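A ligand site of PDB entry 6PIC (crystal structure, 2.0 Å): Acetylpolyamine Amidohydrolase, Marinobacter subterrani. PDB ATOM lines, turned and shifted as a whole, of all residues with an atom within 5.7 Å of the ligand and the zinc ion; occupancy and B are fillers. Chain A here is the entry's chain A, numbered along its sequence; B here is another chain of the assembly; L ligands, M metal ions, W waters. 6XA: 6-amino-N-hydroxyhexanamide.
N of His 163 lies within hydrogen-bond range of OE1 of Glu 325.
The side-chain carboxylate (OD1) of Asp 289 sits close to the backbone NH (N) of Gly 327 (3.5 Å).
O of Gly 172 is in hydrogen-bond range of SG of Cys 174 (3.4 Å).
The side-chain sulfur (SG) of Cys 174 is in hydrogen-bond range of the backbone NH (N) of His 164.
The side-chain carboxylate of Asp 289 sits at hydrogen-bond distance from the backbone NH of Phe 201, 2.8 Å away.
OH of Tyr 173 sits close to OE2 of Glu 22 (3.4 Å).
The side-chain carboxylate (OD1) of Asp 200 lies close to the backbone NH (N) of Gly 326, at 3.0 Å.
OD1 of Asp 122 lies within hydrogen-bond range of N of Gly 172 (3.3 Å).
Of the 22 residues printed, 3 come within 4 Å of the zinc ion.
The nearest printed residue that does not touch the zinc ion is Gly 326 (4.1 Å).
CA of Gly 172 touches C4 of the ligand, 3.7 Å away.
CD2 of Phe 230 touches C5 of the ligand (3.5 Å).
CA of Gly 326 touches O10 of the ligand, 3.97 Å away.
CZ of Phe 96 of chain B touches C2 of the ligand (3.5 Å).
Hydrophobic or aromatic side chains within 4 Å of the ligand: His 163, His 164, Tyr 173, His 202, Phe 230, Tyr 328 and Phe 96 of chain B.
The zinc ion is bound by O9 of the ligand, OD1 of Asp 289, OD2 of Asp 200, ND1 of His 202, O10 of the ligand and OD1 of Asp 200.
The side-chain hydroxyl (OH) of Tyr 328 sits close to an oxygen (O10) of the ligand (2.7 Å).
N8 of the ligand lies within hydrogen-bond range of NE2 of His 163, 3.3 Å away.
NE2 of His 164 lies within hydrogen-bond range of N8 of the ligand.
N1 of the ligand lies within salt-bridge range of OE1 of Glu 22, 3.5 Å away.
A nitrogen (N1) of the ligand lies within salt-bridge range of the side-chain carboxylate (OD2) of Asp 122.
The side-chain hydroxyl of Tyr 173 sits at hydrogen-bond distance from a nitrogen (N1) of the ligand (3.0 Å).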
ATOM      1  N   GLU A  22      -4.736   0.406   3.945  1.00  0.00           N
ATOM      2  CA  GLU A  22      -4.522   1.739   3.399  1.00  0.00           C
ATOM      3  C   GLU A  22      -4.638   1.651   1.886  1.00  0.00           C
ATOM      4  O   GLU A  22      -3.993   0.808   1.267  1.00  0.00           O
ATOM      5  CB  GLU A  22      -3.150   2.306   3.780  1.00  0.00           C
ATOM      6  CG  GLU A  22      -2.775   3.548   2.991  1.00  0.00           C
ATOM      7  CD  GLU A  22      -1.443   4.162   3.406  1.00  0.00           C
ATOM      8  OE1 GLU A  22      -0.847   4.902   2.592  1.00  0.00           O
ATOM      9  OE2 GLU A  22      -0.928   3.802   4.485  1.00  0.00           O
ATOM     10  N   LEU A  23      -5.494   2.496   1.314  1.00  0.00           N
ATOM     11  CA  LEU A  23      -5.607   2.585  -0.137  1.00  0.00           C
ATOM     12  C   LEU A  23      -4.352   3.213  -0.715  1.00  0.00           C
ATOM     13  O   LEU A  23      -4.007   4.360  -0.393  1.00  0.00           O
ATOM     14  CB  LEU A  23      -6.842   3.386  -0.520  1.00  0.00           C
ATOM     15  CG  LEU A  23      -7.106   3.575  -2.023  1.00  0.00           C
ATOM     16  CD1 LEU A  23      -7.214   2.239  -2.736  1.00  0.00           C
ATOM     17  CD2 LEU A  23      -8.359   4.405  -2.259  1.00  0.00           C
ATOM     18  N   ASP A  24      -3.662   2.467  -1.584  1.00  0.00           N
ATOM     19  CA  ASP A  24      -2.436   2.942  -2.229  1.00  0.00           C
ATOM     20  C   ASP A  24      -2.245   2.182  -3.529  1.00  0.00           C
ATOM     21  O   ASP A  24      -2.282   0.953  -3.531  1.00  0.00           O
ATOM     22  CB  ASP A  24      -1.216   2.772  -1.319  1.00  0.00           C
ATOM     23  CG  ASP A  24       0.061   3.246  -1.985  1.00  0.00           C
ATOM     24  OD1 ASP A  24       0.169   4.448  -2.264  1.00  0.00           O
ATOM     25  OD2 ASP A  24       0.966   2.411  -2.227  1.00  0.00           O
ATOM     26  N   ASP A 122      -6.849   7.473   1.908  1.00  0.00           N
ATOM     27  CA  ASP A 122      -5.679   6.757   2.401  1.00  0.00           C
ATOM     28  C   ASP A 122      -5.676   6.588   3.918  1.00  0.00           C
ATOM     29  O   ASP A 122      -4.717   6.035   4.460  1.00  0.00           O
ATOM     30  CB  ASP A 122      -4.407   7.484   1.967  1.00  0.00           C
ATOM     31  CG  ASP A 122      -4.299   8.873   2.550  1.00  0.00           C
ATOM     32  OD1 ASP A 122      -5.309   9.400   3.057  1.00  0.00           O
ATOM     33  OD2 ASP A 122      -3.197   9.464   2.508  1.00  0.00           O
ATOM     34  N   HIS A 163      -0.633  17.485  10.557  1.00  0.00           N
ATOM     35  CA  HIS A 163      -0.514  18.731   9.805  1.00  0.00           C
ATOM     36  C   HIS A 163      -1.366  18.770   8.543  1.00  0.00           C
ATOM     37  O   HIS A 163      -1.485  19.844   7.936  1.00  0.00           O
ATOM     38  CB  HIS A 163       0.948  19.031   9.467  1.00  0.00           C
ATOM     39  CG  HIS A 163       1.562  18.090   8.469  1.00  0.00           C
ATOM     40  ND1 HIS A 163       2.594  18.465   7.633  1.00  0.00           N
ATOM     41  CD2 HIS A 163       1.310  16.787   8.201  1.00  0.00           C
ATOM     42  CE1 HIS A 163       2.932  17.450   6.867  1.00  0.00           C
ATOM     43  NE2 HIS A 163       2.169  16.416   7.196  1.00  0.00           N
ATOM     44  N   HIS A 164      -1.981  17.657   8.131  1.00  0.00           N
ATOM     45  CA  HIS A 164      -2.858  17.654   6.967  1.00  0.00           C
ATOM     46  C   HIS A 164      -4.310  17.961   7.308  1.00  0.00           C
ATOM     47  O   HIS A 164      -5.099  18.215   6.384  1.00  0.00           O
ATOM     48  CB  HIS A 164      -2.789  16.309   6.252  1.00  0.00           C
ATOM     49  CG  HIS A 164      -1.492  16.080   5.527  1.00  0.00           C
ATOM     50  ND1 HIS A 164      -0.972  16.985   4.627  1.00  0.00           N
ATOM     51  CD2 HIS A 164      -0.614  15.044   5.572  1.00  0.00           C
ATOM     52  CE1 HIS A 164       0.170  16.518   4.158  1.00  0.00           C
ATOM     53  NE2 HIS A 164       0.401  15.348   4.707  1.00  0.00           N
ATOM     54  N   GLY A 172      -4.537  12.059   4.775  1.00  0.00           N
ATOM     55  CA  GLY A 172      -3.091  11.946   4.889  1.00  0.00           C
ATOM     56  C   GLY A 172      -2.614  11.475   6.251  1.00  0.00           C
ATOM     57  O   GLY A 172      -1.613  11.992   6.771  1.00  0.00           O
ATOM     58  N   TYR A 173      -3.329  10.525   6.849  1.00  0.00           N
ATOM     59  CA  TYR A 173      -3.006   9.899   8.128  1.00  0.00           C
ATOM     60  C   TYR A 173      -3.254  10.824   9.311  1.00  0.00           C
ATOM     61  O   TYR A 173      -2.837  10.499  10.438  1.00  0.00           O
ATOM     62  CB  TYR A 173      -1.558   9.371   8.188  1.00  0.00           C
ATOM     63  CG  TYR A 173      -1.047   8.666   6.932  1.00  0.00           C
ATOM     64  CD1 TYR A 173      -1.914   8.014   6.066  1.00  0.00           C
ATOM     65  CD2 TYR A 173       0.307   8.653   6.627  1.00  0.00           C
ATOM     66  CE1 TYR A 173      -1.444   7.379   4.921  1.00  0.00           C
ATOM     67  CE2 TYR A 173       0.789   8.012   5.493  1.00  0.00           C
ATOM     68  CZ  TYR A 173      -0.092   7.379   4.644  1.00  0.00           C
ATOM     69  OH  TYR A 173       0.381   6.738   3.520  1.00  0.00           O
ATOM     70  N   CYS A 174      -3.910  11.963   9.102  1.00  0.00           N
ATOM     71  CA  CYS A 174      -4.098  12.983  10.127  1.00  0.00           C
ATOM     72  C   CYS A 174      -5.569  13.147  10.451  1.00  0.00           C
ATOM     73  O   CYS A 174      -6.430  12.986   9.586  1.00  0.00           O
ATOM     74  CB  CYS A 174      -3.520  14.328   9.682  1.00  0.00           C
ATOM     75  SG  CYS A 174      -1.770  14.294   9.218  1.00  0.00           S
ATOM     76  N   ASP A 200       8.362  18.673   7.598  1.00  0.00           N
ATOM     77  CA  ASP A 200       7.965  17.384   7.047  1.00  0.00           C
ATOM     78  C   ASP A 200       8.034  17.465   5.522  1.00  0.00           C
ATOM     79  O   ASP A 200       7.905  18.540   4.936  1.00  0.00           O
ATOM     80  CB  ASP A 200       6.537  17.061   7.520  1.00  0.00           C
ATOM     81  CG  ASP A 200       5.951  15.806   6.887  1.00  0.00           C
ATOM     82  OD1 ASP A 200       5.882  14.775   7.603  1.00  0.00           O
ATOM     83  OD2 ASP A 200       5.586  15.810   5.689  1.00  0.00           O
ATOM     84  N   PHE A 201       8.264  16.328   4.880  1.00  0.00           N
ATOM     85  CA  PHE A 201       8.429  16.329   3.427  1.00  0.00           C
ATOM     86  C   PHE A 201       7.172  16.834   2.717  1.00  0.00           C
ATOM     87  O   PHE A 201       7.270  17.384   1.612  1.00  0.00           O
ATOM     88  CB  PHE A 201       8.801  14.935   2.914  1.00  0.00           C
ATOM     89  CG  PHE A 201       8.641  14.775   1.414  1.00  0.00           C
ATOM     90  CD1 PHE A 201       9.634  15.220   0.547  1.00  0.00           C
ATOM     91  CD2 PHE A 201       7.501  14.190   0.879  1.00  0.00           C
ATOM     92  CE1 PHE A 201       9.498  15.075  -0.835  1.00  0.00           C
ATOM     93  CE2 PHE A 201       7.356  14.044  -0.493  1.00  0.00           C
ATOM     94  CZ  PHE A 201       8.351  14.481  -1.348  1.00  0.00           C
ATOM     95  N   HIS A 202       5.996  16.656   3.313  1.00  0.00           N
ATOM     96  CA  HIS A 202       4.742  17.040   2.694  1.00  0.00           C
ATOM     97  C   HIS A 202       4.268  18.388   3.206  1.00  0.00           C
ATOM     98  O   HIS A 202       4.562  18.794   4.339  1.00  0.00           O
ATOM     99  CB  HIS A 202       3.660  15.988   2.952  1.00  0.00           C
ATOM    100  CG  HIS A 202       4.034  14.606   2.518  1.00  0.00           C
ATOM    101  ND1 HIS A 202       4.689  13.720   3.345  1.00  0.00           N
ATOM    102  CD2 HIS A 202       3.856  13.961   1.340  1.00  0.00           C
ATOM    103  CE1 HIS A 202       4.898  12.587   2.693  1.00  0.00           C
ATOM    104  NE2 HIS A 202       4.399  12.709   1.469  1.00  0.00           N
ATOM    105  N   PHE A 230       1.487  14.353  -2.860  1.00  0.00           N
ATOM    106  CA  PHE A 230       0.468  14.742  -1.885  1.00  0.00           C
ATOM    107  C   PHE A 230       0.908  15.990  -1.135  1.00  0.00           C
ATOM    108  O   PHE A 230       2.091  16.129  -0.792  1.00  0.00           O
ATOM    109  CB  PHE A 230       0.253  13.570  -0.909  1.00  0.00           C
ATOM    110  CG  PHE A 230      -0.870  13.787   0.067  1.00  0.00           C
ATOM    111  CD1 PHE A 230      -2.159  13.369  -0.229  1.00  0.00           C
ATOM    112  CD2 PHE A 230      -0.625  14.385   1.301  1.00  0.00           C
ATOM    113  CE1 PHE A 230      -3.184  13.548   0.680  1.00  0.00           C
ATOM    114  CE2 PHE A 230      -1.650  14.564   2.210  1.00  0.00           C
ATOM    115  CZ  PHE A 230      -2.930  14.145   1.894  1.00  0.00           C
ATOM    116  N   GLY A 287       8.751  16.206  10.472  1.00  0.00           N
ATOM    117  CA  GLY A 287       8.680  14.931   9.758  1.00  0.00           C
ATOM    118  C   GLY A 287      10.064  14.536   9.302  1.00  0.00           C
ATOM    119  O   GLY A 287      10.833  15.372   8.823  1.00  0.00           O
ATOM    120  N   ASP A 289      10.373  12.181   6.940  1.00  0.00           N
ATOM    121  CA  ASP A 289      10.218  11.651   5.591  1.00  0.00           C
ATOM    122  C   ASP A 289      11.054  12.405   4.556  1.00  0.00           C
ATOM    123  O   ASP A 289      11.013  12.045   3.379  1.00  0.00           O
ATOM    124  CB  ASP A 289       8.745  11.625   5.165  1.00  0.00           C
ATOM    125  CG  ASP A 289       7.973  12.833   5.657  1.00  0.00           C
ATOM    126  OD1 ASP A 289       6.747  12.682   5.905  1.00  0.00           O
ATOM    127  OD2 ASP A 289       8.589  13.846   6.025  1.00  0.00           O
ATOM    128  N   ILE A 296       8.225   6.780   0.523  1.00  0.00           N
ATOM    129  CA  ILE A 296       7.170   7.464  -0.221  1.00  0.00           C
ATOM    130  C   ILE A 296       7.536   8.911  -0.546  1.00  0.00           C
ATOM    131  O   ILE A 296       6.674   9.701  -0.926  1.00  0.00           O
ATOM    132  CB  ILE A 296       5.829   7.418   0.549  1.00  0.00           C
ATOM    133  CG1 ILE A 296       5.934   8.191   1.860  1.00  0.00           C
ATOM    134  CG2 ILE A 296       5.394   5.983   0.793  1.00  0.00           C
ATOM    135  CD1 ILE A 296       4.583   8.496   2.493  1.00  0.00           C
ATOM    136  N   GLU A 325       5.340  14.338  13.008  1.00  0.00           N
ATOM    137  CA  GLU A 325       4.468  14.110  11.870  1.00  0.00           C
ATOM    138  C   GLU A 325       4.850  12.830  11.136  1.00  0.00           C
ATOM    139  O   GLU A 325       4.662  11.731  11.674  1.00  0.00           O
ATOM    140  CB  GLU A 325       4.480  15.320  10.924  1.00  0.00           C
ATOM    141  CG  GLU A 325       4.244  16.660  11.604  1.00  0.00           C
ATOM    142  CD  GLU A 325       2.815  16.835  12.128  1.00  0.00           C
ATOM    143  OE1 GLU A 325       1.887  16.214  11.563  1.00  0.00           O
ATOM    144  OE2 GLU A 325       2.620  17.605  13.092  1.00  0.00           O
ATOM    145  N   GLY A 326       5.395  12.943   9.929  1.00  0.00           N
ATOM    146  CA  GLY A 326       5.655  11.803   9.084  1.00  0.00           C
ATOM    147  C   GLY A 326       7.056  11.236   9.233  1.00  0.00           C
ATOM    148  O   GLY A 326       7.848  11.639  10.090  1.00  0.00           O
ATOM    149  N   GLY A 327       7.382  10.284   8.356  1.00  0.00           N
ATOM    150  CA  GLY A 327       8.619   9.519   8.429  1.00  0.00           C
ATOM    151  C   GLY A 327       8.358   8.033   8.474  1.00  0.00           C
ATOM    152  O   GLY A 327       7.743   7.538   9.420  1.00  0.00           O
ATOM    153  N   TYR A 328       8.792   7.283   7.450  1.00  0.00           N
ATOM    154  CA  TYR A 328       8.298   5.930   7.246  1.00  0.00           C
ATOM    155  C   TYR A 328       9.364   4.856   7.019  1.00  0.00           C
ATOM    156  O   TYR A 328       9.003   3.688   6.852  1.00  0.00           O
ATOM    157  CB  TYR A 328       7.288   5.927   6.096  1.00  0.00           C
ATOM    158  CG  TYR A 328       6.197   6.949   6.372  1.00  0.00           C
ATOM    159  CD1 TYR A 328       5.180   6.661   7.275  1.00  0.00           C
ATOM    160  CD2 TYR A 328       6.230   8.211   5.792  1.00  0.00           C
ATOM    161  CE1 TYR A 328       4.192   7.595   7.553  1.00  0.00           C
ATOM    162  CE2 TYR A 328       5.252   9.148   6.069  1.00  0.00           C
ATOM    163  CZ  TYR A 328       4.239   8.837   6.956  1.00  0.00           C
ATOM    164  OH  TYR A 328       3.261   9.773   7.233  1.00  0.00           O
ATOM    165  N   THR B  95      -7.108   8.286  -4.956  1.00  0.00           N
ATOM    166  CA  THR B  95      -6.844   8.251  -3.528  1.00  0.00           C
ATOM    167  C   THR B  95      -6.992   9.611  -2.864  1.00  0.00           C
ATOM    168  O   THR B  95      -7.376   9.678  -1.690  1.00  0.00           O
ATOM    169  CB  THR B  95      -5.432   7.719  -3.244  1.00  0.00           C
ATOM    170  OG1 THR B  95      -5.129   6.643  -4.141  1.00  0.00           O
ATOM    171  CG2 THR B  95      -5.327   7.227  -1.819  1.00  0.00           C
ATOM    172  N   PHE B  96      -6.709  10.694  -3.584  1.00  0.00           N
ATOM    173  CA  PHE B  96      -6.790  12.038  -3.060  1.00  0.00           C
ATOM    174  C   PHE B  96      -7.601  12.895  -4.020  1.00  0.00           C
ATOM    175  O   PHE B  96      -7.677  12.597  -5.206  1.00  0.00           O
ATOM    176  CB  PHE B  96      -5.390  12.653  -2.880  1.00  0.00           C
ATOM    177  CG  PHE B  96      -4.320  11.649  -2.602  1.00  0.00           C
ATOM    178  CD1 PHE B  96      -4.285  10.960  -1.397  1.00  0.00           C
ATOM    179  CD2 PHE B  96      -3.337  11.383  -3.536  1.00  0.00           C
ATOM    180  CE1 PHE B  96      -3.287  10.041  -1.130  1.00  0.00           C
ATOM    181  CE2 PHE B  96      -2.339  10.460  -3.289  1.00  0.00           C
ATOM    182  CZ  PHE B  96      -2.319   9.789  -2.076  1.00  0.00           C
HETATM  183  C2  6XA L   1      -0.178   9.369   0.706  1.00  0.00           C
HETATM  184  C3  6XA L   1       0.623  10.067   1.829  1.00  0.00           C
HETATM  185  C4  6XA L   1      -0.217  11.054   2.683  1.00  0.00           C
HETATM  186  C5  6XA L   1       0.613  12.007   3.592  1.00  0.00           C
HETATM  187  C6  6XA L   1       1.762  11.336   4.412  1.00  0.00           C
HETATM  188  C7  6XA L   1       2.678  12.281   5.199  1.00  0.00           C
HETATM  189  N1  6XA L   1      -0.932   8.140   1.238  1.00  0.00           N
HETATM  190  N8  6XA L   1       2.324  13.580   5.473  1.00  0.00           N
HETATM  191  O10 6XA L   1       3.797  11.836   5.578  1.00  0.00           O
HETATM  192  O9  6XA L   1       3.249  14.338   6.189  1.00  0.00           O
HETATM  193 ZN    ZN M   1       5.050  13.751   5.571  1.00  0.00          ZN
HETATM  194  O   HOH W   1      -1.998   6.028  -0.116  1.00  0.00           O
